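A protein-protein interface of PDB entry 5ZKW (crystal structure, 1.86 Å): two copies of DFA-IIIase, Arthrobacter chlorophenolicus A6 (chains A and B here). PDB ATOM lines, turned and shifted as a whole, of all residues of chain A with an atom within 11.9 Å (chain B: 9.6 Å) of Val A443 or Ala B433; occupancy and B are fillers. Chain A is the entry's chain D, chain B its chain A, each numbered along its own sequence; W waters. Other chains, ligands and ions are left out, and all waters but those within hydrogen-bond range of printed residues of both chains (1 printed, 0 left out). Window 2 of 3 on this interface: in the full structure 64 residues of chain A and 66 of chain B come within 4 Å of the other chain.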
ATOM      1  N   ASP A 402      11.838  29.899  -1.675  1.00  0.00           N
ATOM      2  CA  ASP A 402      13.187  29.554  -2.150  1.00  0.00           C
ATOM      3  C   ASP A 402      13.409  29.983  -3.616  1.00  0.00           C
ATOM      4  O   ASP A 402      12.469  30.100  -4.403  1.00  0.00           O
ATOM      5  CB  ASP A 402      13.489  28.052  -1.956  1.00  0.00           C
ATOM      6  CG  ASP A 402      13.973  27.718  -0.533  1.00  0.00           C
ATOM      7  OD1 ASP A 402      13.983  28.604   0.355  1.00  0.00           O
ATOM      8  OD2 ASP A 402      14.358  26.550  -0.301  1.00  0.00           O
ATOM      9  N   GLY A 423      27.266  23.290  -1.631  1.00  0.00           N
ATOM     10  CA  GLY A 423      26.087  23.153  -2.470  1.00  0.00           C
ATOM     11  C   GLY A 423      25.737  21.695  -2.746  1.00  0.00           C
ATOM     12  O   GLY A 423      26.605  20.809  -2.731  1.00  0.00           O
ATOM     13  N   SER A 424      24.455  21.448  -3.015  1.00  0.00           N
ATOM     14  CA  SER A 424      24.013  20.128  -3.482  1.00  0.00           C
ATOM     15  C   SER A 424      24.581  19.848  -4.878  1.00  0.00           C
ATOM     16  O   SER A 424      25.111  20.746  -5.534  1.00  0.00           O
ATOM     17  CB  SER A 424      22.487  20.065  -3.533  1.00  0.00           C
ATOM     18  OG  SER A 424      22.030  20.919  -4.545  1.00  0.00           O
ATOM     19  N   ASP A 425      24.450  18.615  -5.349  1.00  0.00           N
ATOM     20  CA  ASP A 425      24.935  18.291  -6.697  1.00  0.00           C
ATOM     21  C   ASP A 425      24.352  19.176  -7.793  1.00  0.00           C
ATOM     22  O   ASP A 425      25.089  19.651  -8.664  1.00  0.00           O
ATOM     23  CB  ASP A 425      24.731  16.800  -7.029  1.00  0.00           C
ATOM     24  CG  ASP A 425      25.919  15.955  -6.630  1.00  0.00           C
ATOM     25  OD1 ASP A 425      27.084  16.399  -6.811  1.00  0.00           O
ATOM     26  OD2 ASP A 425      25.691  14.845  -6.127  1.00  0.00           O
ATOM     27  N   THR A 426      23.049  19.434  -7.744  1.00  0.00           N
ATOM     28  CA  THR A 426      22.409  20.286  -8.766  1.00  0.00           C
ATOM     29  C   THR A 426      22.893  21.738  -8.673  1.00  0.00           C
ATOM     30  O   THR A 426      22.930  22.454  -9.675  1.00  0.00           O
ATOM     31  CB  THR A 426      20.865  20.215  -8.685  1.00  0.00           C
ATOM     32  OG1 THR A 426      20.433  20.548  -7.367  1.00  0.00           O
ATOM     33  CG2 THR A 426      20.379  18.819  -8.996  1.00  0.00           C
ATOM     34  N   GLN A 427      23.268  22.163  -7.464  1.00  0.00           N
ATOM     35  CA  GLN A 427      23.790  23.505  -7.238  1.00  0.00           C
ATOM     36  C   GLN A 427      25.241  23.706  -7.661  1.00  0.00           C
ATOM     37  O   GLN A 427      25.669  24.846  -7.767  1.00  0.00           O
ATOM     38  CB  GLN A 427      23.663  23.882  -5.777  1.00  0.00           C
ATOM     39  CG  GLN A 427      22.246  24.168  -5.325  1.00  0.00           C
ATOM     40  CD  GLN A 427      22.202  24.555  -3.866  1.00  0.00           C
ATOM     41  OE1 GLN A 427      22.876  23.951  -3.032  1.00  0.00           O
ATOM     42  NE2 GLN A 427      21.409  25.577  -3.547  1.00  0.00           N
ATOM     43  N   ALA A 439      29.203  16.959  -2.711  1.00  0.00           N
ATOM     44  CA  ALA A 439      27.929  17.632  -2.510  1.00  0.00           C
ATOM     45  C   ALA A 439      27.676  17.783  -1.019  1.00  0.00           C
ATOM     46  O   ALA A 439      28.014  16.887  -0.223  1.00  0.00           O
ATOM     47  CB  ALA A 439      26.808  16.821  -3.138  1.00  0.00           C
ATOM     48  N   THR A 440      27.097  18.916  -0.638  1.00  0.00           N
ATOM     49  CA  THR A 440      26.558  19.060   0.704  1.00  0.00           C
ATOM     50  C   THR A 440      25.506  17.953   0.886  1.00  0.00           C
ATOM     51  O   THR A 440      24.631  17.817   0.033  1.00  0.00           O
ATOM     52  CB  THR A 440      25.908  20.445   0.919  1.00  0.00           C
ATOM     53  OG1 THR A 440      26.867  21.481   0.651  1.00  0.00           O
ATOM     54  CG2 THR A 440      25.411  20.598   2.375  1.00  0.00           C
ATOM     55  N   PRO A 441      25.612  17.148   1.963  1.00  0.00           N
ATOM     56  CA  PRO A 441      24.533  16.206   2.296  1.00  0.00           C
ATOM     57  C   PRO A 441      23.148  16.877   2.358  1.00  0.00           C
ATOM     58  O   PRO A 441      23.018  17.999   2.859  1.00  0.00           O
ATOM     59  CB  PRO A 441      24.940  15.682   3.676  1.00  0.00           C
ATOM     60  CG  PRO A 441      26.423  15.778   3.688  1.00  0.00           C
ATOM     61  CD  PRO A 441      26.742  17.026   2.904  1.00  0.00           C
ATOM     62  N   THR A 442      22.138  16.201   1.810  1.00  0.00           N
ATOM     63  CA  THR A 442      20.762  16.700   1.804  1.00  0.00           C
ATOM     64  C   THR A 442      19.832  15.603   2.306  1.00  0.00           C
ATOM     65  O   THR A 442      20.237  14.453   2.452  1.00  0.00           O
ATOM     66  CB  THR A 442      20.313  17.097   0.383  1.00  0.00           C
ATOM     67  OG1 THR A 442      20.468  15.967  -0.484  1.00  0.00           O
ATOM     68  CG2 THR A 442      21.143  18.246  -0.155  1.00  0.00           C
ATOM     69  N   VAL A 443      18.585  15.972   2.554  1.00  0.00           N
ATOM     70  CA  VAL A 443      17.551  15.011   2.959  1.00  0.00           C
ATOM     71  C   VAL A 443      16.407  15.003   1.946  1.00  0.00           C
ATOM     72  O   VAL A 443      16.227  15.970   1.209  1.00  0.00           O
ATOM     73  CB  VAL A 443      17.038  15.304   4.386  1.00  0.00           C
ATOM     74  CG1 VAL A 443      16.557  16.751   4.542  1.00  0.00           C
ATOM     75  CG2 VAL A 443      15.960  14.306   4.773  1.00  0.00           C
ATOM     76  N   GLY B 366      16.730  25.379   7.872  1.00  0.00           N
ATOM     77  CA  GLY B 366      17.829  25.714   6.969  1.00  0.00           C
ATOM     78  C   GLY B 366      19.133  26.172   7.602  1.00  0.00           C
ATOM     79  O   GLY B 366      19.969  26.755   6.914  1.00  0.00           O
ATOM     80  N   SER B 414      12.506  22.660  15.112  1.00  0.00           N
ATOM     81  CA  SER B 414      13.478  23.068  14.097  1.00  0.00           C
ATOM     82  C   SER B 414      13.711  21.911  13.123  1.00  0.00           C
ATOM     83  O   SER B 414      13.843  20.781  13.553  1.00  0.00           O
ATOM     84  CB  SER B 414      14.803  23.451  14.757  1.00  0.00           C
ATOM     85  OG  SER B 414      15.752  23.871  13.788  1.00  0.00           O
ATOM     86  N   ALA B 415      13.759  22.182  11.820  1.00  0.00           N
ATOM     87  CA  ALA B 415      13.939  21.102  10.839  1.00  0.00           C
ATOM     88  C   ALA B 415      14.615  21.573   9.561  1.00  0.00           C
ATOM     89  O   ALA B 415      14.818  22.765   9.353  1.00  0.00           O
ATOM     90  CB  ALA B 415      12.599  20.427  10.518  1.00  0.00           C
ATOM     91  N   ARG B 416      14.965  20.617   8.711  1.00  0.00           N
ATOM     92  CA  ARG B 416      15.647  20.894   7.440  1.00  0.00           C
ATOM     93  C   ARG B 416      16.961  21.648   7.671  1.00  0.00           C
ATOM     94  O   ARG B 416      17.314  22.556   6.923  1.00  0.00           O
ATOM     95  CB  ARG B 416      14.699  21.605   6.460  1.00  0.00           C
ATOM     96  CG  ARG B 416      13.429  20.785   6.209  1.00  0.00           C
ATOM     97  CD  ARG B 416      12.598  21.293   5.046  1.00  0.00           C
ATOM     98  NE  ARG B 416      11.989  22.600   5.301  1.00  0.00           N
ATOM     99  CZ  ARG B 416      10.840  22.830   5.955  1.00  0.00           C
ATOM    100  NH1 ARG B 416      10.105  21.837   6.480  1.00  0.00           N
ATOM    101  NH2 ARG B 416      10.417  24.088   6.089  1.00  0.00           N
ATOM    102  N   ASN B 417      17.673  21.234   8.716  1.00  0.00           N
ATOM    103  CA  ASN B 417      18.989  21.749   9.035  1.00  0.00           C
ATOM    104  C   ASN B 417      20.027  20.792   8.458  1.00  0.00           C
ATOM    105  O   ASN B 417      19.720  19.644   8.119  1.00  0.00           O
ATOM    106  CB  ASN B 417      19.164  21.867  10.546  1.00  0.00           C
ATOM    107  CG  ASN B 417      18.097  22.745  11.192  1.00  0.00           C
ATOM    108  OD1 ASN B 417      18.045  23.955  10.944  1.00  0.00           O
ATOM    109  ND2 ASN B 417      17.252  22.139  12.037  1.00  0.00           N
ATOM    110  N   THR B 418      21.254  21.288   8.352  1.00  0.00           N
ATOM    111  CA  THR B 418      22.387  20.512   7.857  1.00  0.00           C
ATOM    112  C   THR B 418      23.460  20.568   8.930  1.00  0.00           C
ATOM    113  O   THR B 418      23.897  21.655   9.295  1.00  0.00           O
ATOM    114  CB  THR B 418      22.915  21.111   6.543  1.00  0.00           C
ATOM    115  OG1 THR B 418      21.835  21.183   5.596  1.00  0.00           O
ATOM    116  CG2 THR B 418      24.023  20.273   5.974  1.00  0.00           C
ATOM    117  N   ILE B 419      23.878  19.403   9.415  1.00  0.00           N
ATOM    118  CA  ILE B 419      24.816  19.284  10.537  1.00  0.00           C
ATOM    119  C   ILE B 419      25.985  18.390  10.120  1.00  0.00           C
ATOM    120  O   ILE B 419      25.819  17.182   9.950  1.00  0.00           O
ATOM    121  CB  ILE B 419      24.127  18.717  11.785  1.00  0.00           C
ATOM    122  CG1 ILE B 419      22.968  19.632  12.191  1.00  0.00           C
ATOM    123  CG2 ILE B 419      25.119  18.552  12.933  1.00  0.00           C
ATOM    124  CD1 ILE B 419      21.970  18.967  13.082  1.00  0.00           C
ATOM    125  N   LEU B 420      27.157  19.001   9.954  1.00  0.00           N
ATOM    126  CA  LEU B 420      28.344  18.313   9.428  1.00  0.00           C
ATOM    127  C   LEU B 420      29.510  18.443  10.382  1.00  0.00           C
ATOM    128  O   LEU B 420      29.799  19.541  10.882  1.00  0.00           O
ATOM    129  CB  LEU B 420      28.757  18.901   8.076  1.00  0.00           C
ATOM    130  CG  LEU B 420      27.610  19.161   7.094  1.00  0.00           C
ATOM    131  CD1 LEU B 420      28.128  19.874   5.858  1.00  0.00           C
ATOM    132  CD2 LEU B 420      26.891  17.868   6.733  1.00  0.00           C
ATOM    133  N   ALA B 430      18.893  14.565  16.938  1.00  0.00           N
ATOM    134  CA  ALA B 430      18.112  15.157  15.841  1.00  0.00           C
ATOM    135  C   ALA B 430      17.374  14.090  15.057  1.00  0.00           C
ATOM    136  O   ALA B 430      17.860  12.960  14.909  1.00  0.00           O
ATOM    137  CB  ALA B 430      19.028  15.918  14.883  1.00  0.00           C
ATOM    138  N   ASP B 431      16.210  14.463  14.537  1.00  0.00           N
ATOM    139  CA  ASP B 431      15.460  13.598  13.623  1.00  0.00           C
ATOM    140  C   ASP B 431      16.235  13.464  12.294  1.00  0.00           C
ATOM    141  O   ASP B 431      16.299  14.415  11.526  1.00  0.00           O
ATOM    142  CB  ASP B 431      14.069  14.189  13.399  1.00  0.00           C
ATOM    143  CG  ASP B 431      13.128  13.245  12.666  1.00  0.00           C
ATOM    144  OD1 ASP B 431      13.591  12.292  12.013  1.00  0.00           O
ATOM    145  OD2 ASP B 431      11.911  13.480  12.741  1.00  0.00           O
ATOM    146  N   ARG B 432      16.803  12.284  12.036  1.00  0.00           N
ATOM    147  CA  ARG B 432      17.515  12.007  10.771  1.00  0.00           C
ATOM    148  C   ARG B 432      16.622  12.063   9.528  1.00  0.00           C
ATOM    149  O   ARG B 432      17.130  12.240   8.413  1.00  0.00           O
ATOM    150  CB  ARG B 432      18.232  10.639  10.808  1.00  0.00           C
ATOM    151  CG  ARG B 432      19.671  10.693  11.289  1.00  0.00           C
ATOM    152  CD  ARG B 432      19.757  11.126  12.738  1.00  0.00           C
ATOM    153  NE  ARG B 432      21.124  11.023  13.260  1.00  0.00           N
ATOM    154  CZ  ARG B 432      21.538  11.502  14.433  1.00  0.00           C
ATOM    155  NH1 ARG B 432      20.709  12.148  15.245  1.00  0.00           N
ATOM    156  NH2 ARG B 432      22.812  11.352  14.791  1.00  0.00           N
ATOM    157  N   ALA B 433      15.313  11.890   9.695  1.00  0.00           N
ATOM    158  CA  ALA B 433      14.393  11.948   8.545  1.00  0.00           C
ATOM    159  C   ALA B 433      14.217  13.337   7.928  1.00  0.00           C
ATOM    160  O   ALA B 433      13.834  13.445   6.759  1.00  0.00           O
ATOM    161  CB  ALA B 433      13.030  11.368   8.910  1.00  0.00           C
ATOM    162  N   VAL B 434      14.442  14.394   8.711  1.00  0.00           N
ATOM    163  CA  VAL B 434      14.215  15.766   8.247  1.00  0.00           C
ATOM    164  C   VAL B 434      15.402  16.717   8.459  1.00  0.00           C
ATOM    165  O   VAL B 434      15.260  17.917   8.256  1.00  0.00           O
ATOM    166  CB  VAL B 434      12.937  16.367   8.869  1.00  0.00           C
ATOM    167  CG1 VAL B 434      11.705  15.608   8.374  1.00  0.00           C
ATOM    168  CG2 VAL B 434      13.014  16.376  10.394  1.00  0.00           C
ATOM    169  N   ASN B 435      16.559  16.183   8.833  1.00  0.00           N
ATOM    170  CA  ASN B 435      17.796  16.957   8.915  1.00  0.00           C
ATOM    171  C   ASN B 435      18.891  16.142   8.252  1.00  0.00           C
ATOM    172  O   ASN B 435      18.902  14.912   8.381  1.00  0.00           O
ATOM    173  CB  ASN B 435      18.179  17.214  10.374  1.00  0.00           C
ATOM    174  CG  ASN B 435      17.133  18.014  11.124  1.00  0.00           C
ATOM    175  OD1 ASN B 435      17.072  19.241  11.002  1.00  0.00           O
ATOM    176  ND2 ASN B 435      16.295  17.317  11.909  1.00  0.00           N
ATOM    177  N   ALA B 436      19.810  16.819   7.561  1.00  0.00           N
ATOM    178  CA  ALA B 436      20.934  16.153   6.893  1.00  0.00           C
ATOM    179  C   ALA B 436      22.106  16.135   7.855  1.00  0.00           C
ATOM    180  O   ALA B 436      22.636  17.193   8.212  1.00  0.00           O
ATOM    181  CB  ALA B 436      21.316  16.881   5.619  1.00  0.00           C
ATOM    182  N   ILE B 437      22.508  14.944   8.275  1.00  0.00           N
ATOM    183  CA  ILE B 437      23.531  14.790   9.304  1.00  0.00           C
ATOM    184  C   ILE B 437      24.723  13.983   8.811  1.00  0.00           C
ATOM    185  O   ILE B 437      24.557  12.864   8.321  1.00  0.00           O
ATOM    186  CB  ILE B 437      22.946  14.136  10.555  1.00  0.00           C
ATOM    187  CG1 ILE B 437      21.827  15.019  11.123  1.00  0.00           C
ATOM    188  CG2 ILE B 437      24.030  13.909  11.611  1.00  0.00           C
ATOM    189  CD1 ILE B 437      20.872  14.227  11.977  1.00  0.00           C
HETATM  190  O   HOH W   1      21.490  20.057   3.209  1.00  0.00           O
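The backbone carbonyl oxygen (O) of Asn B417 lies within hydrogen-bond range of the backbone NH (N) of Ala B436 (2.9 Å). The backbone NH (N) of Ala B433 lies within hydrogen-bond range of the side-chain carboxylate (OD1) of Asp B431 (2.9 Å). The backbone NH of Ile B419 is in hydrogen-bond range of the backbone carbonyl oxygen of Ala B436 (2.8 Å). The backbone carbonyl oxygen (O) of Gly A423 sits at hydrogen-bond distance from the backbone NH (N) of Thr A440 (2.9 Å).
Thr B418 touches Thr A440 (CG2 to CG2, 3.9 Å). Pro A441 touches Thr B418 (O to CG2, 3.99 Å). Pro A441 touches Leu B420. CB of Ala B436 touches O of Pro A441, at 3.4 Å. Thr A442 touches Ala B436. Val A443 touches Ala B433.
Of the printed residues of chain B, Thr A440 touches Thr B418. Of the printed residues of chain B, Pro A441 touches Thr B418 (3.99 Å), Leu B420 (3.7 Å) and Ala B436 (3.4 Å). Thr A442 touches one residue of chain B. Of chain B, only Ala B433 (3.0 Å) comes within 4 Å of Val A443. Of the printed residues of chain A, Thr B418 touches Thr A440 (3.9 Å) and Pro A441 (3.99 Å). Printed residues of chain A within 4 Å of Leu B420: Pro A441 (3.7 Å). No residue of chain A comes within 4 Å of Asp B431. Of chain A, only Val A443 comes within 4 Å of Ala B433. Ala B436 touches just these residues of chain A: Pro A441 and Thr A442. The nearest printed residue of chain B that does not touch Thr A440 is Leu B420 (4.5 Å).
Along chain A the printed residues that touch a printed residue of chain B span positions 440 to 443. Of the 16 printed residues of chain B, 4 touch a printed residue of chain A. Hydrophobic or aromatic side chains of chain B within 4 Å of the printed part of chain A: Leu B420 and Ala B436.
No position is printed for both chains.
Water W1 lies within hydrogen-bond range of the backbone carbonyl oxygen (O) of Pro A441 (2.6 Å) and the side-chain hydroxyl (OG1) of Thr B418 (2.7 Å).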
